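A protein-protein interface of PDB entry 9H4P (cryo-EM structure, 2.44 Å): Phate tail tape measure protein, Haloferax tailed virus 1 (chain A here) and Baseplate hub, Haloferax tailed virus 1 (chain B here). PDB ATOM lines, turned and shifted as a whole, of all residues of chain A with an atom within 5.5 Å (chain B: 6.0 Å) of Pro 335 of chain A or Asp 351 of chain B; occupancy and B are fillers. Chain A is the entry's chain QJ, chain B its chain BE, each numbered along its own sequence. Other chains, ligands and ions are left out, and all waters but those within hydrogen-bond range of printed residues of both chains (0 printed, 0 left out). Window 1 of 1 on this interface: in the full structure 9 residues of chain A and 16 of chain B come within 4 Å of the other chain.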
ATOM      1  N   TYR A 331       7.958  34.797  23.882  1.00  0.00           N
ATOM      2  CA  TYR A 331       8.235  33.377  23.695  1.00  0.00           C
ATOM      3  C   TYR A 331       7.714  32.520  24.859  1.00  0.00           C
ATOM      4  O   TYR A 331       7.257  31.404  24.615  1.00  0.00           O
ATOM      5  CB  TYR A 331       9.725  33.165  23.399  1.00  0.00           C
ATOM      6  CG  TYR A 331      10.282  33.984  22.256  1.00  0.00           C
ATOM      7  CD1 TYR A 331       9.792  33.842  20.963  1.00  0.00           C
ATOM      8  CD2 TYR A 331      11.306  34.901  22.459  1.00  0.00           C
ATOM      9  CE1 TYR A 331      10.304  34.579  19.905  1.00  0.00           C
ATOM     10  CE2 TYR A 331      11.829  35.648  21.412  1.00  0.00           C
ATOM     11  CZ  TYR A 331      11.326  35.487  20.131  1.00  0.00           C
ATOM     12  OH  TYR A 331      11.831  36.220  19.098  1.00  0.00           O
ATOM     13  N   ARG A 332       7.770  33.023  26.109  1.00  0.00           N
ATOM     14  CA  ARG A 332       7.307  32.284  27.285  1.00  0.00           C
ATOM     15  C   ARG A 332       5.796  32.026  27.245  1.00  0.00           C
ATOM     16  O   ARG A 332       5.342  30.966  27.679  1.00  0.00           O
ATOM     17  CB  ARG A 332       7.651  33.007  28.593  1.00  0.00           C
ATOM     18  CG  ARG A 332       9.135  33.061  28.935  1.00  0.00           C
ATOM     19  CD  ARG A 332       9.391  33.363  30.405  1.00  0.00           C
ATOM     20  NE  ARG A 332       8.522  34.406  30.952  1.00  0.00           N
ATOM     21  CZ  ARG A 332       8.716  35.720  30.851  1.00  0.00           C
ATOM     22  NH1 ARG A 332       7.841  36.555  31.386  1.00  0.00           N
ATOM     23  NH2 ARG A 332       9.775  36.203  30.223  1.00  0.00           N
ATOM     24  N   SER A 333       5.035  33.006  26.733  1.00  0.00           N
ATOM     25  CA  SER A 333       3.581  32.959  26.633  1.00  0.00           C
ATOM     26  C   SER A 333       3.104  32.142  25.428  1.00  0.00           C
ATOM     27  O   SER A 333       1.925  31.795  25.365  1.00  0.00           O
ATOM     28  CB  SER A 333       2.995  34.360  26.612  1.00  0.00           C
ATOM     29  OG  SER A 333       3.487  35.110  25.508  1.00  0.00           O
ATOM     30  N   ASP A 334       4.012  31.835  24.485  1.00  0.00           N
ATOM     31  CA  ASP A 334       3.670  31.268  23.183  1.00  0.00           C
ATOM     32  C   ASP A 334       2.967  29.908  23.280  1.00  0.00           C
ATOM     33  O   ASP A 334       1.943  29.732  22.616  1.00  0.00           O
ATOM     34  CB  ASP A 334       4.881  31.246  22.246  1.00  0.00           C
ATOM     35  CG  ASP A 334       4.554  30.798  20.835  1.00  0.00           C
ATOM     36  OD1 ASP A 334       3.599  31.343  20.251  1.00  0.00           O
ATOM     37  OD2 ASP A 334       5.266  29.912  20.334  1.00  0.00           O
ATOM     38  N   PRO A 335       3.470  28.902  24.054  1.00  0.00           N
ATOM     39  CA  PRO A 335       2.807  27.595  24.144  1.00  0.00           C
ATOM     40  C   PRO A 335       1.355  27.670  24.617  1.00  0.00           C
ATOM     41  O   PRO A 335       0.527  26.874  24.179  1.00  0.00           O
ATOM     42  CB  PRO A 335       3.657  26.800  25.153  1.00  0.00           C
ATOM     43  CG  PRO A 335       5.016  27.467  25.101  1.00  0.00           C
ATOM     44  CD  PRO A 335       4.706  28.931  24.864  1.00  0.00           C
ATOM     45  N   SER A 336       1.064  28.632  25.505  1.00  0.00           N
ATOM     46  CA  SER A 336      -0.274  28.815  26.046  1.00  0.00           C
ATOM     47  C   SER A 336      -1.211  29.421  24.999  1.00  0.00           C
ATOM     48  O   SER A 336      -2.364  29.004  24.912  1.00  0.00           O
ATOM     49  CB  SER A 336      -0.260  29.583  27.346  1.00  0.00           C
ATOM     50  OG  SER A 336       0.615  28.977  28.287  1.00  0.00           O
ATOM     51  N   ARG A 337      -0.706  30.370  24.191  1.00  0.00           N
ATOM     52  CA  ARG A 337      -1.447  30.919  23.060  1.00  0.00           C
ATOM     53  C   ARG A 337      -1.729  29.829  22.021  1.00  0.00           C
ATOM     54  O   ARG A 337      -2.836  29.778  21.484  1.00  0.00           O
ATOM     55  CB  ARG A 337      -0.755  32.152  22.465  1.00  0.00           C
ATOM     56  CG  ARG A 337      -1.214  33.480  23.056  1.00  0.00           C
ATOM     57  CD  ARG A 337      -1.084  33.600  24.568  1.00  0.00           C
ATOM     58  NE  ARG A 337      -1.382  34.933  25.072  1.00  0.00           N
ATOM     59  CZ  ARG A 337      -2.586  35.400  25.396  1.00  0.00           C
ATOM     60  NH1 ARG A 337      -2.699  36.639  25.839  1.00  0.00           N
ATOM     61  NH2 ARG A 337      -3.668  34.650  25.283  1.00  0.00           N
ATOM     62  N   ARG A 338      -0.742  28.949  21.778  1.00  0.00           N
ATOM     63  CA  ARG A 338      -0.877  27.785  20.907  1.00  0.00           C
ATOM     64  C   ARG A 338      -1.974  26.830  21.393  1.00  0.00           C
ATOM     65  O   ARG A 338      -2.591  26.146  20.574  1.00  0.00           O
ATOM     66  CB  ARG A 338       0.472  27.076  20.754  1.00  0.00           C
ATOM     67  CG  ARG A 338       1.342  27.640  19.640  1.00  0.00           C
ATOM     68  CD  ARG A 338       2.829  27.673  19.938  1.00  0.00           C
ATOM     69  NE  ARG A 338       3.350  26.412  20.458  1.00  0.00           N
ATOM     70  CZ  ARG A 338       4.536  26.238  21.038  1.00  0.00           C
ATOM     71  NH1 ARG A 338       4.888  25.040  21.471  1.00  0.00           N
ATOM     72  NH2 ARG A 338       5.376  27.250  21.175  1.00  0.00           N
ATOM     73  N   ARG A 339      -2.224  26.806  22.715  1.00  0.00           N
ATOM     74  CA  ARG A 339      -3.248  25.972  23.337  1.00  0.00           C
ATOM     75  C   ARG A 339      -4.525  26.755  23.668  1.00  0.00           C
ATOM     76  O   ARG A 339      -5.342  26.289  24.464  1.00  0.00           O
ATOM     77  CB  ARG A 339      -2.662  25.233  24.545  1.00  0.00           C
ATOM     78  CG  ARG A 339      -1.648  24.173  24.149  1.00  0.00           C
ATOM     79  CD  ARG A 339      -0.881  23.668  25.344  1.00  0.00           C
ATOM     80  NE  ARG A 339      -1.596  22.680  26.141  1.00  0.00           N
ATOM     81  CZ  ARG A 339      -1.093  22.090  27.219  1.00  0.00           C
ATOM     82  NH1 ARG A 339      -1.802  21.194  27.883  1.00  0.00           N
ATOM     83  NH2 ARG A 339       0.125  22.390  27.633  1.00  0.00           N
ATOM     84  N   GLY A 340      -4.713  27.918  23.027  1.00  0.00           N
ATOM     85  CA  GLY A 340      -5.880  28.759  23.249  1.00  0.00           C
ATOM     86  C   GLY A 340      -5.665  29.753  24.389  1.00  0.00           C
ATOM     87  O   GLY A 340      -5.263  30.889  24.142  1.00  0.00           O
ATOM     88  N   PHE B  50      -1.515  19.892  22.291  1.00  0.00           N
ATOM     89  CA  PHE B  50      -0.540  20.905  21.894  1.00  0.00           C
ATOM     90  C   PHE B  50      -0.805  21.411  20.476  1.00  0.00           C
ATOM     91  O   PHE B  50      -1.300  20.678  19.625  1.00  0.00           O
ATOM     92  CB  PHE B  50       0.872  20.318  22.005  1.00  0.00           C
ATOM     93  CG  PHE B  50       1.131  19.578  23.292  1.00  0.00           C
ATOM     94  CD1 PHE B  50       1.433  20.276  24.473  1.00  0.00           C
ATOM     95  CD2 PHE B  50       0.978  18.184  23.322  1.00  0.00           C
ATOM     96  CE1 PHE B  50       1.526  19.582  25.688  1.00  0.00           C
ATOM     97  CE2 PHE B  50       1.074  17.490  24.535  1.00  0.00           C
ATOM     98  CZ  PHE B  50       1.324  18.195  25.718  1.00  0.00           C
ATOM     99  N   GLY B  51      -0.496  22.676  20.214  1.00  0.00           N
ATOM    100  CA  GLY B  51      -0.729  23.290  18.907  1.00  0.00           C
ATOM    101  C   GLY B  51       0.375  22.992  17.899  1.00  0.00           C
ATOM    102  O   GLY B  51       1.547  23.165  18.215  1.00  0.00           O
ATOM    103  N   GLY B 348       4.411  18.878  29.575  1.00  0.00           N
ATOM    104  CA  GLY B 348       5.371  19.659  30.361  1.00  0.00           C
ATOM    105  C   GLY B 348       5.169  21.175  30.312  1.00  0.00           C
ATOM    106  O   GLY B 348       4.266  21.681  29.652  1.00  0.00           O
ATOM    107  N   ASP B 349       6.088  21.891  30.969  1.00  0.00           N
ATOM    108  CA  ASP B 349       6.191  23.360  31.053  1.00  0.00           C
ATOM    109  C   ASP B 349       5.098  24.046  31.909  1.00  0.00           C
ATOM    110  O   ASP B 349       4.088  23.449  32.272  1.00  0.00           O
ATOM    111  CB  ASP B 349       6.332  23.926  29.621  1.00  0.00           C
ATOM    112  CG  ASP B 349       6.967  25.315  29.518  1.00  0.00           C
ATOM    113  OD1 ASP B 349       7.367  25.871  30.559  1.00  0.00           O
ATOM    114  OD2 ASP B 349       7.064  25.834  28.385  1.00  0.00           O
ATOM    115  N   VAL B 350       5.280  25.326  32.258  1.00  0.00           N
ATOM    116  CA  VAL B 350       4.300  26.130  33.029  1.00  0.00           C
ATOM    117  C   VAL B 350       2.981  26.297  32.279  1.00  0.00           C
ATOM    118  O   VAL B 350       1.930  26.522  32.856  1.00  0.00           O
ATOM    119  CB  VAL B 350       4.906  27.491  33.415  1.00  0.00           C
ATOM    120  CG1 VAL B 350       5.053  28.437  32.227  1.00  0.00           C
ATOM    121  CG2 VAL B 350       4.082  28.221  34.472  1.00  0.00           C
ATOM    122  N   ASP B 351       3.035  26.088  30.980  1.00  0.00           N
ATOM    123  CA  ASP B 351       1.915  25.955  30.076  1.00  0.00           C
ATOM    124  C   ASP B 351       0.878  24.889  30.486  1.00  0.00           C
ATOM    125  O   ASP B 351      -0.330  25.101  30.382  1.00  0.00           O
ATOM    126  CB  ASP B 351       2.570  25.558  28.762  1.00  0.00           C
ATOM    127  CG  ASP B 351       1.544  25.429  27.663  1.00  0.00           C
ATOM    128  OD1 ASP B 351       0.640  26.289  27.631  1.00  0.00           O
ATOM    129  OD2 ASP B 351       1.682  24.471  26.872  1.00  0.00           O
ATOM    130  N   ASP B 352       1.311  23.744  31.016  1.00  0.00           N
ATOM    131  CA  ASP B 352       0.367  22.771  31.566  1.00  0.00           C
ATOM    132  C   ASP B 352      -0.321  23.300  32.824  1.00  0.00           C
ATOM    133  O   ASP B 352      -1.512  23.089  32.992  1.00  0.00           O
ATOM    134  CB  ASP B 352       1.047  21.427  31.842  1.00  0.00           C
ATOM    135  CG  ASP B 352       1.075  20.494  30.623  1.00  0.00           C
ATOM    136  OD1 ASP B 352       0.268  20.681  29.682  1.00  0.00           O
ATOM    137  OD2 ASP B 352       1.860  19.526  30.639  1.00  0.00           O
ATOM    138  N   ILE B 353       0.380  24.039  33.680  1.00  0.00           N
ATOM    139  CA  ILE B 353      -0.238  24.653  34.855  1.00  0.00           C
ATOM    140  C   ILE B 353      -1.266  25.697  34.418  1.00  0.00           C
ATOM    141  O   ILE B 353      -2.403  25.667  34.871  1.00  0.00           O
ATOM    142  CB  ILE B 353       0.817  25.264  35.791  1.00  0.00           C
ATOM    143  CG1 ILE B 353       1.803  24.193  36.284  1.00  0.00           C
ATOM    144  CG2 ILE B 353       0.123  25.951  36.976  1.00  0.00           C
ATOM    145  CD1 ILE B 353       3.052  24.775  36.924  1.00  0.00           C
ATOM    146  N   LEU B 354      -0.901  26.594  33.504  1.00  0.00           N
ATOM    147  CA  LEU B 354      -1.811  27.621  33.013  1.00  0.00           C
ATOM    148  C   LEU B 354      -3.026  27.022  32.313  1.00  0.00           C
ATOM    149  O   LEU B 354      -4.139  27.477  32.550  1.00  0.00           O
ATOM    150  CB  LEU B 354      -1.073  28.570  32.066  1.00  0.00           C
ATOM    151  CG  LEU B 354      -0.058  29.483  32.760  1.00  0.00           C
ATOM    152  CD1 LEU B 354       0.780  30.218  31.722  1.00  0.00           C
ATOM    153  CD2 LEU B 354      -0.754  30.516  33.638  1.00  0.00           C
ATOM    154  N   SER B 355      -2.864  25.988  31.496  1.00  0.00           N
ATOM    155  CA  SER B 355      -4.001  25.358  30.824  1.00  0.00           C
ATOM    156  C   SER B 355      -4.895  24.555  31.774  1.00  0.00           C
ATOM    157  O   SER B 355      -6.109  24.584  31.591  1.00  0.00           O
ATOM    158  CB  SER B 355      -3.544  24.510  29.649  1.00  0.00           C
ATOM    159  OG  SER B 355      -2.615  23.547  30.062  1.00  0.00           O
ATOM    160  N   GLU B 356      -4.378  23.915  32.824  1.00  0.00           N
ATOM    161  CA  GLU B 356      -5.238  23.286  33.835  1.00  0.00           C
ATOM    162  C   GLU B 356      -5.996  24.311  34.678  1.00  0.00           C
ATOM    163  O   GLU B 356      -7.171  24.105  34.975  1.00  0.00           O
ATOM    164  CB  GLU B 356      -4.436  22.362  34.763  1.00  0.00           C
ATOM    165  CG  GLU B 356      -3.898  21.082  34.106  1.00  0.00           C
ATOM    166  CD  GLU B 356      -5.000  20.121  33.633  1.00  0.00           C
ATOM    167  OE1 GLU B 356      -5.630  20.389  32.585  1.00  0.00           O
ATOM    168  OE2 GLU B 356      -5.211  19.072  34.288  1.00  0.00           O
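OD1 of Asp 351 of chain B lies within hydrogen-bond range of OG of Ser 336 of chain A. NH2 of Arg 339 of chain A is in salt-bridge range of OD2 of Asp 351 of chain B (2.7 Å). The guanidinium group (NH1) of Arg 339 of chain A lies within hydrogen-bond range of the side-chain hydroxyl (OG) of Ser 355 of chain B (3.3 Å). OD1 of Asp 352 of chain B is in salt-bridge range of NH2 of Arg 339 of chain A (2.7 Å).
Printed residues of chain B that touch a printed residue of chain A: Phe 50, Gly 51, Asp 351, Asp 352, Leu 354 and Ser 355. Along chain B the printed residues that touch a printed residue of chain A span positions 50 to 355. Of the 10 printed residues of chain A, 4 touch a printed residue of chain B. Hydrophobic or aromatic side chains of chain A within 4 Å of the printed part of chain B: Pro 335. Along chain A the printed residues that touch a printed residue of chain B span positions 335 to 339. Among the printed residues, Asp or Glu carboxylates within 4 Å of a Lys or Arg side-chain nitrogen of the other chain: Arg 339 of chain A with Asp 351 of chain B (2.7 Å) and Arg 339 of chain A with Asp 352 of chain B (2.7 Å).
Among the printed residues, merely in contact across the chains: Pro 335 of chain A with Asp 351 of chain B (3.4 Å), Ser 336 of chain A with Leu 354 of chain B (3.7 Å), Arg 339 of chain A with Phe 50 of chain B (3.7 Å) and Arg 338 of chain A with Gly 51 of chain B (3.8 Å).
Of chain B, only Asp 351 comes within 4 Å of Pro 335 of chain A. Asp 351 of chain B touches just these residues of chain A: Pro 335 (3.4 Å), Ser 336 (2.8 Å) and Arg 339 (2.7 Å). Printed residues of chain B within 4 Å of Arg 339 of chain A: Phe 50, Asp 351, Asp 352 and Ser 355. Printed residues of chain A within 4 Å of Phe 50 of chain B: Arg 339 (3.7 Å). Of the printed residues of chain A, Ser 355 of chain B touches Arg 339. Printed residues of chain B within 4 Å of Ser 336 of chain A: Asp 351 (2.8 Å) and Leu 354 (3.7 Å). Of the printed residues of chain A, Leu 354 of chain B touches Ser 336. Arg 332 of chain A touches none of the printed residues of chain B. Asp 349 of chain B touches none of the printed residues of chain A. The nearest residue of chain B that does not touch Pro 335 of chain A is Asp 349 of chain B (4.2 Å). The nearest printed residue of chain A that does not touch Asp 351 of chain B is Arg 337 of chain A (5.5 Å). The nearest printed residue of chain A that does not touch Asp 352 of chain B is Ser 336 of chain A (5.9 Å).
The backbone carbonyl oxygen (O) of Asp 351 of chain B sits at hydrogen-bond distance from the side-chain hydroxyl (OG) of Ser 355 of chain B (2.8 Å). The side-chain hydroxyl (OG) of Ser 355 of chain B sits at hydrogen-bond distance from the backbone carbonyl oxygen (O) of Asp 352 of chain B, 3.2 Å away. The guanidinium group (NH2) of Arg 338 of chain A is in salt-bridge range of the side-chain carboxylate (OD2) of Asp 334 of chain A, 2.8 Å away. The side-chain carboxylate (OD2) of Asp 352 of chain B lies within hydrogen-bond range of the backbone NH (N) of Gly 348 of chain B (2.8 Å).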
